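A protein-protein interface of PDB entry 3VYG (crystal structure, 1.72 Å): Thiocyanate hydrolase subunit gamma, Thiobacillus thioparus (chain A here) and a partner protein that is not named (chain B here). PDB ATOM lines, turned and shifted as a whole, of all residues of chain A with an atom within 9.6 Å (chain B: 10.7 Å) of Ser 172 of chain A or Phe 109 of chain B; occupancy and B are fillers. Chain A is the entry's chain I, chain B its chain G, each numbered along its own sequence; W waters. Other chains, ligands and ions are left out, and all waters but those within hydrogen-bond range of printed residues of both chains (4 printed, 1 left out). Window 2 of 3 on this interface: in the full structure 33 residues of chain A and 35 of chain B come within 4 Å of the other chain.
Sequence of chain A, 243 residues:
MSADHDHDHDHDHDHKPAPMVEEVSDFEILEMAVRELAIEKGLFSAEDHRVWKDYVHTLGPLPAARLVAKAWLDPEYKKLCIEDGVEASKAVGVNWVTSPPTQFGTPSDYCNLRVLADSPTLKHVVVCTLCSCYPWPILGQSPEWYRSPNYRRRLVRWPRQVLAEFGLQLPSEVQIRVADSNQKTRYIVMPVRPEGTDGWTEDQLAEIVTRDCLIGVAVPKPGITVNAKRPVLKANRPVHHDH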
ATOM      1  N   PRO A 120       0.960  21.611  -1.922  1.00  0.00           N
ATOM      2  CA  PRO A 120       2.264  21.315  -1.370  1.00  0.00           C
ATOM      3  C   PRO A 120       2.621  19.856  -1.628  1.00  0.00           C
ATOM      4  O   PRO A 120       3.816  19.515  -1.410  1.00  0.00           O
ATOM      5  CB  PRO A 120       2.055  21.515   0.131  1.00  0.00           C
ATOM      6  CG  PRO A 120       0.989  22.688   0.129  1.00  0.00           C
ATOM      7  CD  PRO A 120       0.034  22.187  -0.913  1.00  0.00           C
ATOM      8  N   THR A 121       1.678  19.016  -2.041  1.00  0.00           N
ATOM      9  CA  THR A 121       2.098  17.610  -2.333  1.00  0.00           C
ATOM     10  C   THR A 121       1.923  17.184  -3.769  1.00  0.00           C
ATOM     11  O   THR A 121       1.991  15.996  -4.057  1.00  0.00           O
ATOM     12  CB  THR A 121       1.299  16.647  -1.475  1.00  0.00           C
ATOM     13  OG1 THR A 121      -0.176  16.789  -1.683  1.00  0.00           O
ATOM     14  CG2 THR A 121       1.673  16.831   0.013  1.00  0.00           C
ATOM     15  N   ARG A 157       8.342  10.461 -19.446  1.00  0.00           N
ATOM     16  CA  ARG A 157       8.992   9.304 -18.889  1.00  0.00           C
ATOM     17  C   ARG A 157      10.149   9.751 -17.881  1.00  0.00           C
ATOM     18  O   ARG A 157      10.418   8.965 -16.922  1.00  0.00           O
ATOM     19  CB  ARG A 157       9.701   8.555 -20.098  1.00  0.00           C
ATOM     20  CG  ARG A 157      10.366   7.273 -19.566  1.00  0.00           C
ATOM     21  CD  ARG A 157      10.662   6.360 -20.781  1.00  0.00           C
ATOM     22  NE  ARG A 157      11.102   5.055 -20.263  1.00  0.00           N
ATOM     23  CZ  ARG A 157      11.044   3.920 -20.980  1.00  0.00           C
ATOM     24  NH1 ARG A 157      10.649   3.957 -22.276  1.00  0.00           N
ATOM     25  NH2 ARG A 157      11.316   2.755 -20.403  1.00  0.00           N
ATOM     26  N   TRP A 158      10.783  10.896 -18.095  1.00  0.00           N
ATOM     27  CA  TRP A 158      11.816  11.462 -17.164  1.00  0.00           C
ATOM     28  C   TRP A 158      11.480  12.877 -16.767  1.00  0.00           C
ATOM     29  O   TRP A 158      12.202  13.791 -17.060  1.00  0.00           O
ATOM     30  CB  TRP A 158      13.191  11.463 -17.876  1.00  0.00           C
ATOM     31  CG  TRP A 158      13.614  10.033 -18.320  1.00  0.00           C
ATOM     32  CD1 TRP A 158      14.148   9.025 -17.537  1.00  0.00           C
ATOM     33  CD2 TRP A 158      13.516   9.482 -19.665  1.00  0.00           C
ATOM     34  NE1 TRP A 158      14.335   7.885 -18.302  1.00  0.00           N
ATOM     35  CE2 TRP A 158      13.974   8.164 -19.608  1.00  0.00           C
ATOM     36  CE3 TRP A 158      13.061  10.009 -20.927  1.00  0.00           C
ATOM     37  CZ2 TRP A 158      14.052   7.304 -20.792  1.00  0.00           C
ATOM     38  CZ3 TRP A 158      13.075   9.128 -22.126  1.00  0.00           C
ATOM     39  CH2 TRP A 158      13.541   7.798 -22.010  1.00  0.00           C
ATOM     40  N   PRO A 159      10.269  13.075 -16.194  1.00  0.00           N
ATOM     41  CA  PRO A 159       9.880  14.487 -15.956  1.00  0.00           C
ATOM     42  C   PRO A 159      10.770  15.206 -14.967  1.00  0.00           C
ATOM     43  O   PRO A 159      11.014  16.406 -15.171  1.00  0.00           O
ATOM     44  CB  PRO A 159       8.435  14.348 -15.388  1.00  0.00           C
ATOM     45  CG  PRO A 159       8.354  12.976 -14.807  1.00  0.00           C
ATOM     46  CD  PRO A 159       9.195  12.140 -15.891  1.00  0.00           C
ATOM     47  N   ARG A 160      11.243  14.523 -13.924  1.00  0.00           N
ATOM     48  CA  ARG A 160      12.129  15.229 -12.937  1.00  0.00           C
ATOM     49  C   ARG A 160      13.443  15.631 -13.582  1.00  0.00           C
ATOM     50  O   ARG A 160      13.935  16.704 -13.364  1.00  0.00           O
ATOM     51  CB  ARG A 160      12.387  14.285 -11.782  1.00  0.00           C
ATOM     52  CG  ARG A 160      11.053  14.188 -10.940  1.00  0.00           C
ATOM     53  CD  ARG A 160      11.289  13.684  -9.672  1.00  0.00           C
ATOM     54  NE  ARG A 160      10.040  13.481  -8.927  1.00  0.00           N
ATOM     55  CZ  ARG A 160       9.739  14.145  -7.808  1.00  0.00           C
ATOM     56  NH1 ARG A 160      10.515  15.092  -7.359  1.00  0.00           N
ATOM     57  NH2 ARG A 160       8.657  13.765  -7.127  1.00  0.00           N
ATOM     58  N   GLN A 161      13.926  14.784 -14.506  1.00  0.00           N
ATOM     59  CA  GLN A 161      15.138  15.152 -15.309  1.00  0.00           C
ATOM     60  C   GLN A 161      14.961  16.287 -16.238  1.00  0.00           C
ATOM     61  O   GLN A 161      15.831  17.155 -16.264  1.00  0.00           O
ATOM     62  CB  GLN A 161      15.720  13.873 -16.022  1.00  0.00           C
ATOM     63  CG  GLN A 161      16.030  12.646 -14.955  1.00  0.00           C
ATOM     64  CD  GLN A 161      14.895  11.705 -14.645  1.00  0.00           C
ATOM     65  OE1 GLN A 161      13.754  12.081 -14.767  1.00  0.00           O
ATOM     66  NE2 GLN A 161      15.188  10.477 -14.246  1.00  0.00           N
ATOM     67  N   ALA A 164      14.462  19.490 -14.157  1.00  0.00           N
ATOM     68  CA  ALA A 164      15.709  19.992 -13.592  1.00  0.00           C
ATOM     69  C   ALA A 164      16.506  20.823 -14.598  1.00  0.00           C
ATOM     70  O   ALA A 164      17.139  21.843 -14.208  1.00  0.00           O
ATOM     71  CB  ALA A 164      16.510  18.808 -12.967  1.00  0.00           C
ATOM     72  N   GLN A 169      13.347  21.706  -9.310  1.00  0.00           N
ATOM     73  CA  GLN A 169      13.366  20.405  -8.620  1.00  0.00           C
ATOM     74  C   GLN A 169      12.352  20.503  -7.466  1.00  0.00           C
ATOM     75  O   GLN A 169      12.156  21.623  -6.843  1.00  0.00           O
ATOM     76  CB  GLN A 169      14.749  20.169  -7.992  1.00  0.00           C
ATOM     77  CG  GLN A 169      15.787  19.667  -8.939  1.00  0.00           C
ATOM     78  CD  GLN A 169      17.111  19.266  -8.225  1.00  0.00           C
ATOM     79  OE1 GLN A 169      17.427  19.776  -7.139  1.00  0.00           O
ATOM     80  NE2 GLN A 169      17.924  18.394  -8.890  1.00  0.00           N
ATOM     81  N   LEU A 170      11.713  19.360  -7.154  1.00  0.00           N
ATOM     82  CA  LEU A 170      10.757  19.227  -6.042  1.00  0.00           C
ATOM     83  C   LEU A 170      11.185  18.124  -5.108  1.00  0.00           C
ATOM     84  O   LEU A 170      11.828  17.143  -5.568  1.00  0.00           O
ATOM     85  CB  LEU A 170       9.367  18.871  -6.608  1.00  0.00           C
ATOM     86  CG  LEU A 170       8.852  20.239  -7.130  1.00  0.00           C
ATOM     87  CD1 LEU A 170       8.633  20.442  -8.561  1.00  0.00           C
ATOM     88  CD2 LEU A 170       7.833  20.903  -6.143  1.00  0.00           C
ATOM     89  N   PRO A 171      10.702  18.140  -3.830  1.00  0.00           N
ATOM     90  CA  PRO A 171      10.976  17.032  -2.928  1.00  0.00           C
ATOM     91  C   PRO A 171      10.569  15.670  -3.561  1.00  0.00           C
ATOM     92  O   PRO A 171       9.588  15.618  -4.373  1.00  0.00           O
ATOM     93  CB  PRO A 171      10.055  17.308  -1.741  1.00  0.00           C
ATOM     94  CG  PRO A 171      10.088  18.840  -1.716  1.00  0.00           C
ATOM     95  CD  PRO A 171       9.856  19.173  -3.164  1.00  0.00           C
ATOM     96  N   SER A 172      11.281  14.608  -3.209  1.00  0.00           N
ATOM     97  CA  SER A 172      10.961  13.363  -3.815  1.00  0.00           C
ATOM     98  C   SER A 172       9.604  12.780  -3.423  1.00  0.00           C
ATOM     99  O   SER A 172       9.029  11.931  -4.128  1.00  0.00           O
ATOM    100  CB  SER A 172      12.102  12.356  -3.558  1.00  0.00           C
ATOM    101  OG  SER A 172      12.223  12.215  -2.166  1.00  0.00           O
ATOM    102  N   GLU A 173       9.032  13.263  -2.332  1.00  0.00           N
ATOM    103  CA  GLU A 173       7.775  12.675  -1.890  1.00  0.00           C
ATOM    104  C   GLU A 173       6.633  13.495  -2.553  1.00  0.00           C
ATOM    105  O   GLU A 173       5.522  13.028  -2.559  1.00  0.00           O
ATOM    106  CB  GLU A 173       7.667  12.626  -0.345  1.00  0.00           C
ATOM    107  CG  GLU A 173       7.604  14.010   0.290  1.00  0.00           C
ATOM    108  CD  GLU A 173       8.933  14.674   0.700  1.00  0.00           C
ATOM    109  OE1 GLU A 173      10.098  14.294   0.205  1.00  0.00           O
ATOM    110  OE2 GLU A 173       8.760  15.625   1.559  1.00  0.00           O
ATOM    111  N   VAL A 174       6.930  14.686  -3.083  1.00  0.00           N
ATOM    112  CA  VAL A 174       5.884  15.459  -3.834  1.00  0.00           C
ATOM    113  C   VAL A 174       5.515  14.664  -5.081  1.00  0.00           C
ATOM    114  O   VAL A 174       6.385  14.159  -5.769  1.00  0.00           O
ATOM    115  CB  VAL A 174       6.436  16.826  -4.201  1.00  0.00           C
ATOM    116  CG1 VAL A 174       5.548  17.556  -5.294  1.00  0.00           C
ATOM    117  CG2 VAL A 174       6.502  17.681  -2.913  1.00  0.00           C
ATOM    118  N   GLN A 175       4.213  14.570  -5.419  1.00  0.00           N
ATOM    119  CA  GLN A 175       3.742  13.838  -6.598  1.00  0.00           C
ATOM    120  C   GLN A 175       3.946  14.800  -7.756  1.00  0.00           C
ATOM    121  O   GLN A 175       3.259  15.854  -7.859  1.00  0.00           O
ATOM    122  CB  GLN A 175       2.223  13.540  -6.436  1.00  0.00           C
ATOM    123  CG  GLN A 175       1.610  13.029  -7.731  1.00  0.00           C
ATOM    124  CD  GLN A 175       0.118  12.743  -7.604  1.00  0.00           C
ATOM    125  OE1 GLN A 175      -0.478  12.740  -6.474  1.00  0.00           O
ATOM    126  NE2 GLN A 175      -0.459  12.451  -8.683  1.00  0.00           N
ATOM    127  N   ILE A 176       4.880  14.521  -8.675  1.00  0.00           N
ATOM    128  CA  ILE A 176       4.892  15.229  -9.923  1.00  0.00           C
ATOM    129  C   ILE A 176       3.929  14.524 -10.866  1.00  0.00           C
ATOM    130  O   ILE A 176       3.991  13.271 -11.063  1.00  0.00           O
ATOM    131  CB  ILE A 176       6.331  15.177 -10.620  1.00  0.00           C
ATOM    132  CG1 ILE A 176       7.344  15.868  -9.719  1.00  0.00           C
ATOM    133  CG2 ILE A 176       6.181  15.733 -12.060  1.00  0.00           C
ATOM    134  CD1 ILE A 176       7.199  17.349  -9.604  1.00  0.00           C
ATOM    135  N   ARG A 177       2.937  15.258 -11.404  1.00  0.00           N
ATOM    136  CA  ARG A 177       1.985  14.648 -12.334  1.00  0.00           C
ATOM    137  C   ARG A 177       2.212  15.299 -13.686  1.00  0.00           C
ATOM    138  O   ARG A 177       2.121  16.544 -13.872  1.00  0.00           O
ATOM    139  CB  ARG A 177       0.515  14.889 -11.857  1.00  0.00           C
ATOM    140  CG  ARG A 177      -0.477  14.553 -12.977  1.00  0.00           C
ATOM    141  CD  ARG A 177      -1.952  14.483 -12.388  1.00  0.00           C
ATOM    142  NE  ARG A 177      -2.118  13.494 -11.330  1.00  0.00           N
ATOM    143  CZ  ARG A 177      -3.227  13.321 -10.613  1.00  0.00           C
ATOM    144  NH1 ARG A 177      -3.209  12.565  -9.545  1.00  0.00           N
ATOM    145  NH2 ARG A 177      -4.336  13.962 -10.990  1.00  0.00           N
ATOM    146  N   PHE B  96      -2.291   7.308 -14.097  1.00  0.00           N
ATOM    147  CA  PHE B  96      -1.418   6.129 -13.925  1.00  0.00           C
ATOM    148  C   PHE B  96      -0.281   6.427 -13.007  1.00  0.00           C
ATOM    149  O   PHE B  96       0.236   7.551 -13.008  1.00  0.00           O
ATOM    150  CB  PHE B  96      -0.786   5.752 -15.311  1.00  0.00           C
ATOM    151  CG  PHE B  96      -1.810   5.433 -16.396  1.00  0.00           C
ATOM    152  CD1 PHE B  96      -2.311   4.133 -16.492  1.00  0.00           C
ATOM    153  CD2 PHE B  96      -2.293   6.450 -17.293  1.00  0.00           C
ATOM    154  CE1 PHE B  96      -3.218   3.822 -17.513  1.00  0.00           C
ATOM    155  CE2 PHE B  96      -3.316   6.122 -18.284  1.00  0.00           C
ATOM    156  CZ  PHE B  96      -3.717   4.819 -18.364  1.00  0.00           C
ATOM    157  N   ALA B  97       0.154   5.419 -12.211  1.00  0.00           N
ATOM    158  CA  ALA B  97       1.402   5.634 -11.553  1.00  0.00           C
ATOM    159  C   ALA B  97       2.585   5.463 -12.511  1.00  0.00           C
ATOM    160  O   ALA B  97       2.538   4.559 -13.362  1.00  0.00           O
ATOM    161  CB  ALA B  97       1.573   4.494 -10.444  1.00  0.00           C
ATOM    162  N   GLN B  98       3.582   6.367 -12.449  1.00  0.00           N
ATOM    163  CA  GLN B  98       4.700   6.323 -13.361  1.00  0.00           C
ATOM    164  C   GLN B  98       5.401   4.982 -13.278  1.00  0.00           C
ATOM    165  O   GLN B  98       5.841   4.490 -14.304  1.00  0.00           O
ATOM    166  CB  GLN B  98       5.689   7.428 -13.062  1.00  0.00           C
ATOM    167  CG  GLN B  98       5.208   8.813 -13.490  1.00  0.00           C
ATOM    168  CD  GLN B  98       5.319   9.051 -15.006  1.00  0.00           C
ATOM    169  OE1 GLN B  98       5.029   8.178 -15.803  1.00  0.00           O
ATOM    170  NE2 GLN B  98       5.696  10.238 -15.369  1.00  0.00           N
ATOM    171  N   LYS B  99       5.385   4.382 -12.094  1.00  0.00           N
ATOM    172  CA  LYS B  99       6.045   3.060 -11.916  1.00  0.00           C
ATOM    173  C   LYS B  99       5.391   1.963 -12.739  1.00  0.00           C
ATOM    174  O   LYS B  99       6.034   0.938 -13.048  1.00  0.00           O
ATOM    175  CB  LYS B  99       6.109   2.749 -10.394  1.00  0.00           C
ATOM    176  CG  LYS B  99       4.746   2.344  -9.821  1.00  0.00           C
ATOM    177  N   ASP B 100       4.098   2.138 -13.080  1.00  0.00           N
ATOM    178  CA  ASP B 100       3.353   1.161 -13.842  1.00  0.00           C
ATOM    179  C   ASP B 100       3.536   1.359 -15.331  1.00  0.00           C
ATOM    180  O   ASP B 100       3.255   0.426 -16.112  1.00  0.00           O
ATOM    181  CB  ASP B 100       1.826   1.231 -13.531  1.00  0.00           C
ATOM    182  CG  ASP B 100       1.526   0.656 -12.137  1.00  0.00           C
ATOM    183  OD1 ASP B 100       2.380  -0.139 -11.566  1.00  0.00           O
ATOM    184  OD2 ASP B 100       0.508   1.012 -11.532  1.00  0.00           O
ATOM    185  N   LEU B 101       4.104   2.459 -15.727  1.00  0.00           N
ATOM    186  CA  LEU B 101       4.366   2.696 -17.131  1.00  0.00           C
ATOM    187  C   LEU B 101       5.841   2.339 -17.503  1.00  0.00           C
ATOM    188  O   LEU B 101       6.112   1.712 -18.532  1.00  0.00           O
ATOM    189  CB  LEU B 101       4.237   4.205 -17.393  1.00  0.00           C
ATOM    190  CG  LEU B 101       2.716   4.577 -17.215  1.00  0.00           C
ATOM    191  CD1 LEU B 101       2.654   6.111 -17.641  1.00  0.00           C
ATOM    192  CD2 LEU B 101       1.752   3.813 -18.169  1.00  0.00           C
ATOM    193  N   TRP B 102       6.770   2.792 -16.646  1.00  0.00           N
ATOM    194  CA  TRP B 102       8.225   2.735 -16.979  1.00  0.00           C
ATOM    195  C   TRP B 102       8.930   1.870 -15.964  1.00  0.00           C
ATOM    196  O   TRP B 102       9.017   2.215 -14.773  1.00  0.00           O
ATOM    197  CB  TRP B 102       8.816   4.166 -16.938  1.00  0.00           C
ATOM    198  CG  TRP B 102       7.926   5.175 -17.571  1.00  0.00           C
ATOM    199  CD1 TRP B 102       7.301   6.232 -16.905  1.00  0.00           C
ATOM    200  CD2 TRP B 102       7.526   5.259 -18.953  1.00  0.00           C
ATOM    201  NE1 TRP B 102       6.524   6.984 -17.820  1.00  0.00           N
ATOM    202  CE2 TRP B 102       6.665   6.454 -19.074  1.00  0.00           C
ATOM    203  CE3 TRP B 102       7.800   4.494 -20.108  1.00  0.00           C
ATOM    204  CZ2 TRP B 102       6.056   6.808 -20.269  1.00  0.00           C
ATOM    205  CZ3 TRP B 102       7.209   4.875 -21.326  1.00  0.00           C
ATOM    206  CH2 TRP B 102       6.354   6.040 -21.393  1.00  0.00           C
ATOM    207  N   GLU B 104      11.888   1.240 -15.162  1.00  0.00           N
ATOM    208  CA  GLU B 104      13.086   1.834 -14.518  1.00  0.00           C
ATOM    209  C   GLU B 104      12.788   2.925 -13.503  1.00  0.00           C
ATOM    210  O   GLU B 104      13.659   3.487 -12.867  1.00  0.00           O
ATOM    211  CB  GLU B 104      14.098   2.332 -15.589  1.00  0.00           C
ATOM    212  CG  GLU B 104      13.801   3.663 -16.283  1.00  0.00           C
ATOM    213  CD  GLU B 104      12.671   3.621 -17.334  1.00  0.00           C
ATOM    214  OE1 GLU B 104      12.110   2.500 -17.669  1.00  0.00           O
ATOM    215  OE2 GLU B 104      12.388   4.747 -17.831  1.00  0.00           O
ATOM    216  N   TYR B 105      11.537   3.265 -13.409  1.00  0.00           N
ATOM    217  CA  TYR B 105      11.223   4.497 -12.659  1.00  0.00           C
ATOM    218  C   TYR B 105      11.688   4.266 -11.243  1.00  0.00           C
ATOM    219  O   TYR B 105      11.381   3.227 -10.670  1.00  0.00           O
ATOM    220  CB  TYR B 105       9.661   4.785 -12.671  1.00  0.00           C
ATOM    221  CG  TYR B 105       9.390   6.276 -12.558  1.00  0.00           C
ATOM    222  CD1 TYR B 105       9.485   7.081 -13.698  1.00  0.00           C
ATOM    223  CD2 TYR B 105       9.038   6.849 -11.347  1.00  0.00           C
ATOM    224  CE1 TYR B 105       9.326   8.511 -13.641  1.00  0.00           C
ATOM    225  CE2 TYR B 105       8.821   8.233 -11.272  1.00  0.00           C
ATOM    226  CZ  TYR B 105       9.003   9.028 -12.355  1.00  0.00           C
ATOM    227  OH  TYR B 105       8.823  10.405 -12.321  1.00  0.00           O
ATOM    228  N   SER B 106      12.277   5.315 -10.623  1.00  0.00           N
ATOM    229  CA  SER B 106      12.872   5.121  -9.280  1.00  0.00           C
ATOM    230  C   SER B 106      11.802   5.014  -8.164  1.00  0.00           C
ATOM    231  O   SER B 106      10.884   5.777  -8.148  1.00  0.00           O
ATOM    232  CB  SER B 106      13.852   6.263  -8.957  1.00  0.00           C
ATOM    233  OG  SER B 106      14.354   5.986  -7.635  1.00  0.00           O
ATOM    234  N   ASP B 107      11.933   4.025  -7.262  1.00  0.00           N
ATOM    235  CA  ASP B 107      11.078   4.023  -6.065  1.00  0.00           C
ATOM    236  C   ASP B 107      11.194   5.268  -5.238  1.00  0.00           C
ATOM    237  O   ASP B 107      10.306   5.503  -4.395  1.00  0.00           O
ATOM    238  CB  ASP B 107      11.509   2.904  -5.089  1.00  0.00           C
ATOM    239  CG  ASP B 107      11.222   1.523  -5.577  1.00  0.00           C
ATOM    240  OD1 ASP B 107      10.506   1.310  -6.581  1.00  0.00           O
ATOM    241  OD2 ASP B 107      11.767   0.616  -4.884  1.00  0.00           O
ATOM    242  N   THR B 108      12.272   6.039  -5.373  1.00  0.00           N
ATOM    243  CA  THR B 108      12.422   7.250  -4.539  1.00  0.00           C
ATOM    244  C   THR B 108      11.324   8.264  -4.929  1.00  0.00           C
ATOM    245  O   THR B 108      10.846   9.050  -4.063  1.00  0.00           O
ATOM    246  CB  THR B 108      13.766   7.887  -4.796  1.00  0.00           C
ATOM    247  OG1 THR B 108      14.732   6.989  -4.282  1.00  0.00           O
ATOM    248  CG2 THR B 108      13.854   9.213  -4.062  1.00  0.00           C
ATOM    249  N   PHE B 109      10.963   8.212  -6.219  1.00  0.00           N
ATOM    250  CA  PHE B 109       9.890   9.079  -6.774  1.00  0.00           C
ATOM    251  C   PHE B 109       8.536   8.330  -6.822  1.00  0.00           C
ATOM    252  O   PHE B 109       7.856   8.310  -7.833  1.00  0.00           O
ATOM    253  CB  PHE B 109      10.350   9.627  -8.122  1.00  0.00           C
ATOM    254  CG  PHE B 109      11.679  10.326  -8.066  1.00  0.00           C
ATOM    255  CD1 PHE B 109      11.960  11.317  -7.099  1.00  0.00           C
ATOM    256  CD2 PHE B 109      12.620  10.108  -9.049  1.00  0.00           C
ATOM    257  CE1 PHE B 109      13.229  11.999  -7.072  1.00  0.00           C
ATOM    258  CE2 PHE B 109      13.890  10.762  -9.001  1.00  0.00           C
ATOM    259  CZ  PHE B 109      14.195  11.721  -8.050  1.00  0.00           C
ATOM    260  N   ALA B 110       8.182   7.882  -5.615  1.00  0.00           N
ATOM    261  CA  ALA B 110       7.111   6.891  -5.255  1.00  0.00           C
ATOM    262  C   ALA B 110       5.729   7.355  -5.756  1.00  0.00           C
ATOM    263  O   ALA B 110       4.934   6.580  -6.244  1.00  0.00           O
ATOM    264  CB  ALA B 110       7.081   6.732  -3.691  1.00  0.00           C
ATOM    265  N   ASN B 111       5.506   8.650  -5.723  1.00  0.00           N
ATOM    266  CA  ASN B 111       4.179   9.105  -5.919  1.00  0.00           C
ATOM    267  C   ASN B 111       3.902   9.721  -7.282  1.00  0.00           C
ATOM    268  O   ASN B 111       2.775  10.195  -7.483  1.00  0.00           O
ATOM    269  CB  ASN B 111       3.816  10.148  -4.789  1.00  0.00           C
ATOM    270  CG  ASN B 111       4.074   9.605  -3.416  1.00  0.00           C
ATOM    271  OD1 ASN B 111       4.631  10.299  -2.533  1.00  0.00           O
ATOM    272  ND2 ASN B 111       3.563   8.393  -3.173  1.00  0.00           N
ATOM    273  N   ASP B 112       4.875   9.707  -8.199  1.00  0.00           N
ATOM    274  CA  ASP B 112       4.723  10.449  -9.489  1.00  0.00           C
ATOM    275  C   ASP B 112       3.711   9.727 -10.371  1.00  0.00           C
ATOM    276  O   ASP B 112       3.575   8.510 -10.348  1.00  0.00           O
ATOM    277  CB  ASP B 112       6.066  10.586 -10.247  1.00  0.00           C
ATOM    278  CG  ASP B 112       7.059  11.501  -9.556  1.00  0.00           C
ATOM    279  OD1 ASP B 112       6.694  12.204  -8.533  1.00  0.00           O
ATOM    280  OD2 ASP B 112       8.219  11.610 -10.081  1.00  0.00           O
ATOM    281  N   THR B 113       2.941  10.525 -11.141  1.00  0.00           N
ATOM    282  CA  THR B 113       1.866   9.985 -11.921  1.00  0.00           C
ATOM    283  C   THR B 113       1.816  10.661 -13.307  1.00  0.00           C
ATOM    284  O   THR B 113       2.504  11.666 -13.599  1.00  0.00           O
ATOM    285  CB  THR B 113       0.498  10.295 -11.289  1.00  0.00           C
ATOM    286  OG1 THR B 113       0.414  11.720 -11.042  1.00  0.00           O
ATOM    287  CG2 THR B 113       0.380   9.542  -9.963  1.00  0.00           C
ATOM    288  N   LEU B 114       0.992  10.082 -14.152  1.00  0.00           N
ATOM    289  CA  LEU B 114       0.737  10.623 -15.527  1.00  0.00           C
ATOM    290  C   LEU B 114      -0.782  10.605 -15.716  1.00  0.00           C
ATOM    291  O   LEU B 114      -1.411   9.551 -15.453  1.00  0.00           O
ATOM    292  CB  LEU B 114       1.412   9.688 -16.565  1.00  0.00           C
ATOM    293  CG  LEU B 114       1.281  10.281 -18.001  1.00  0.00           C
ATOM    294  CD1 LEU B 114       2.526  10.034 -18.762  1.00  0.00           C
ATOM    295  CD2 LEU B 114      -0.036   9.609 -18.673  1.00  0.00           C
HETATM  296  O   HOH W   1       5.268  12.256 -13.214  1.00  0.00           O
HETATM  297  O   HOH W   2      11.275  11.761 -13.224  1.00  0.00           O
HETATM  298  O   HOH W   3      13.235   0.320 -18.964  1.00  0.00           O
HETATM  299  O   HOH W   4      11.913   6.793 -16.048  1.00  0.00           O
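Arg 157 of chain A touches Trp 102 of chain B (NE to CE3, 3.4 Å).
Pro 159 of chain A touches Gln 98 of chain B.
Pro 159 of chain A touches Tyr 105 of chain B.
Arg 160 of chain A touches Phe 109 of chain B (NE to CD1, 3.4 Å).
Asn 111 of chain B touches Gln 175 of chain A (O to CG, 3.1 Å).
Asp 112 of chain B touches Gln 175 of chain A.
The indole nitrogen (NE1) of Trp 102 of chain B is in hydrogen-bond range of the side-chain amide oxygen (OE1) of Gln 98 of chain B (2.8 Å).
The side-chain amide nitrogen (NE2) of Gln 175 of chain A sits close to the guanidinium group (NH1) of Arg 177 of chain A (2.9 Å).
Printed residues of chain B within 4 Å of Trp 158 of chain A: Glu 104.
Printed residues of chain B within 4 Å of Pro 159 of chain A: Gln 98 and Tyr 105.
Of the printed residues of chain B, Arg 160 of chain A touches Phe 109 and Asp 112.
Ser 172 of chain A touches just these residues of chain B: Thr 108 (3.4 Å) and Phe 109 (3.7 Å).
Val 174 of chain A touches just one residue of chain B: Asp 112.
Printed residues of chain A within 4 Å of Trp 102 of chain B: Arg 157 (3.4 Å).
Printed residues of chain A within 4 Å of Thr 108 of chain B: Ser 172.
Of chain A, only Arg 160 (3.4 Å) and Ser 172 (3.7 Å) come within 4 Å of Phe 109 of chain B.
No residue of chain A comes within 4 Å of Ala 110 of chain B.
The nearest residue of chain B that does not touch Ser 172 of chain A is Ala 110 of chain B (4.4 Å).
The nearest residue of chain A that does not touch Phe 109 of chain B is Gln 161 of chain A (5.4 Å).
The nearest printed residue of chain B that does not touch Gln 175 of chain A is Leu 114 of chain B (6.1 Å).
Water W4 lies within hydrogen-bond range of the side-chain carboxylate of Glu 104 of chain B (2.8 Å), the backbone carbonyl oxygen of Arg 157 of chain A (2.8 Å) and the indole nitrogen of Trp 158 of chain A (3.5 Å).
Water W2 lies within hydrogen-bond range of the backbone NH of Arg 160 of chain A, the side-chain amide oxygen of Gln 161 of chain A and the side-chain hydroxyl of Tyr 105 of chain B.
Of the 18 printed residues of chain B, 9 touch a printed residue of chain A.
Among the printed residues, 18 pairs touch across the chains.
The backbone carbonyl oxygen of Val 174 of chain A sits close to the side-chain carboxylate of Asp 112 of chain B.
OD1 of Asp 112 of chain B lies within hydrogen-bond range of N of Ile 176 of chain A (2.9 Å).
The backbone NH (N) of Thr 113 of chain B sits at hydrogen-bond distance from the backbone carbonyl oxygen (O) of Ile 176 of chain A, at 2.9 Å.
The side-chain amide oxygen (OD1) of Asn 111 of chain B sits close to the backbone carbonyl oxygen (O) of Glu 173 of chain A (2.9 Å).
The backbone carbonyl oxygen (O) of Ser 172 of chain A sits close to the backbone carbonyl oxygen (O) of Thr 108 of chain B (3.4 Å).
OG1 of Thr 113 of chain B lies within hydrogen-bond range of NE2 of Gln 175 of chain A (2.6 Å).
The guanidinium group (NE) of Arg 177 of chain A lies within hydrogen-bond range of the side-chain hydroxyl (OG1) of Thr 113 of chain B (3.1 Å).
OE2 of Glu 104 of chain B is in salt-bridge range of NE of Arg 157 of chain A.
NE of Arg 160 of chain A lies within salt-bridge range of OD2 of Asp 112 of chain B (2.9 Å).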
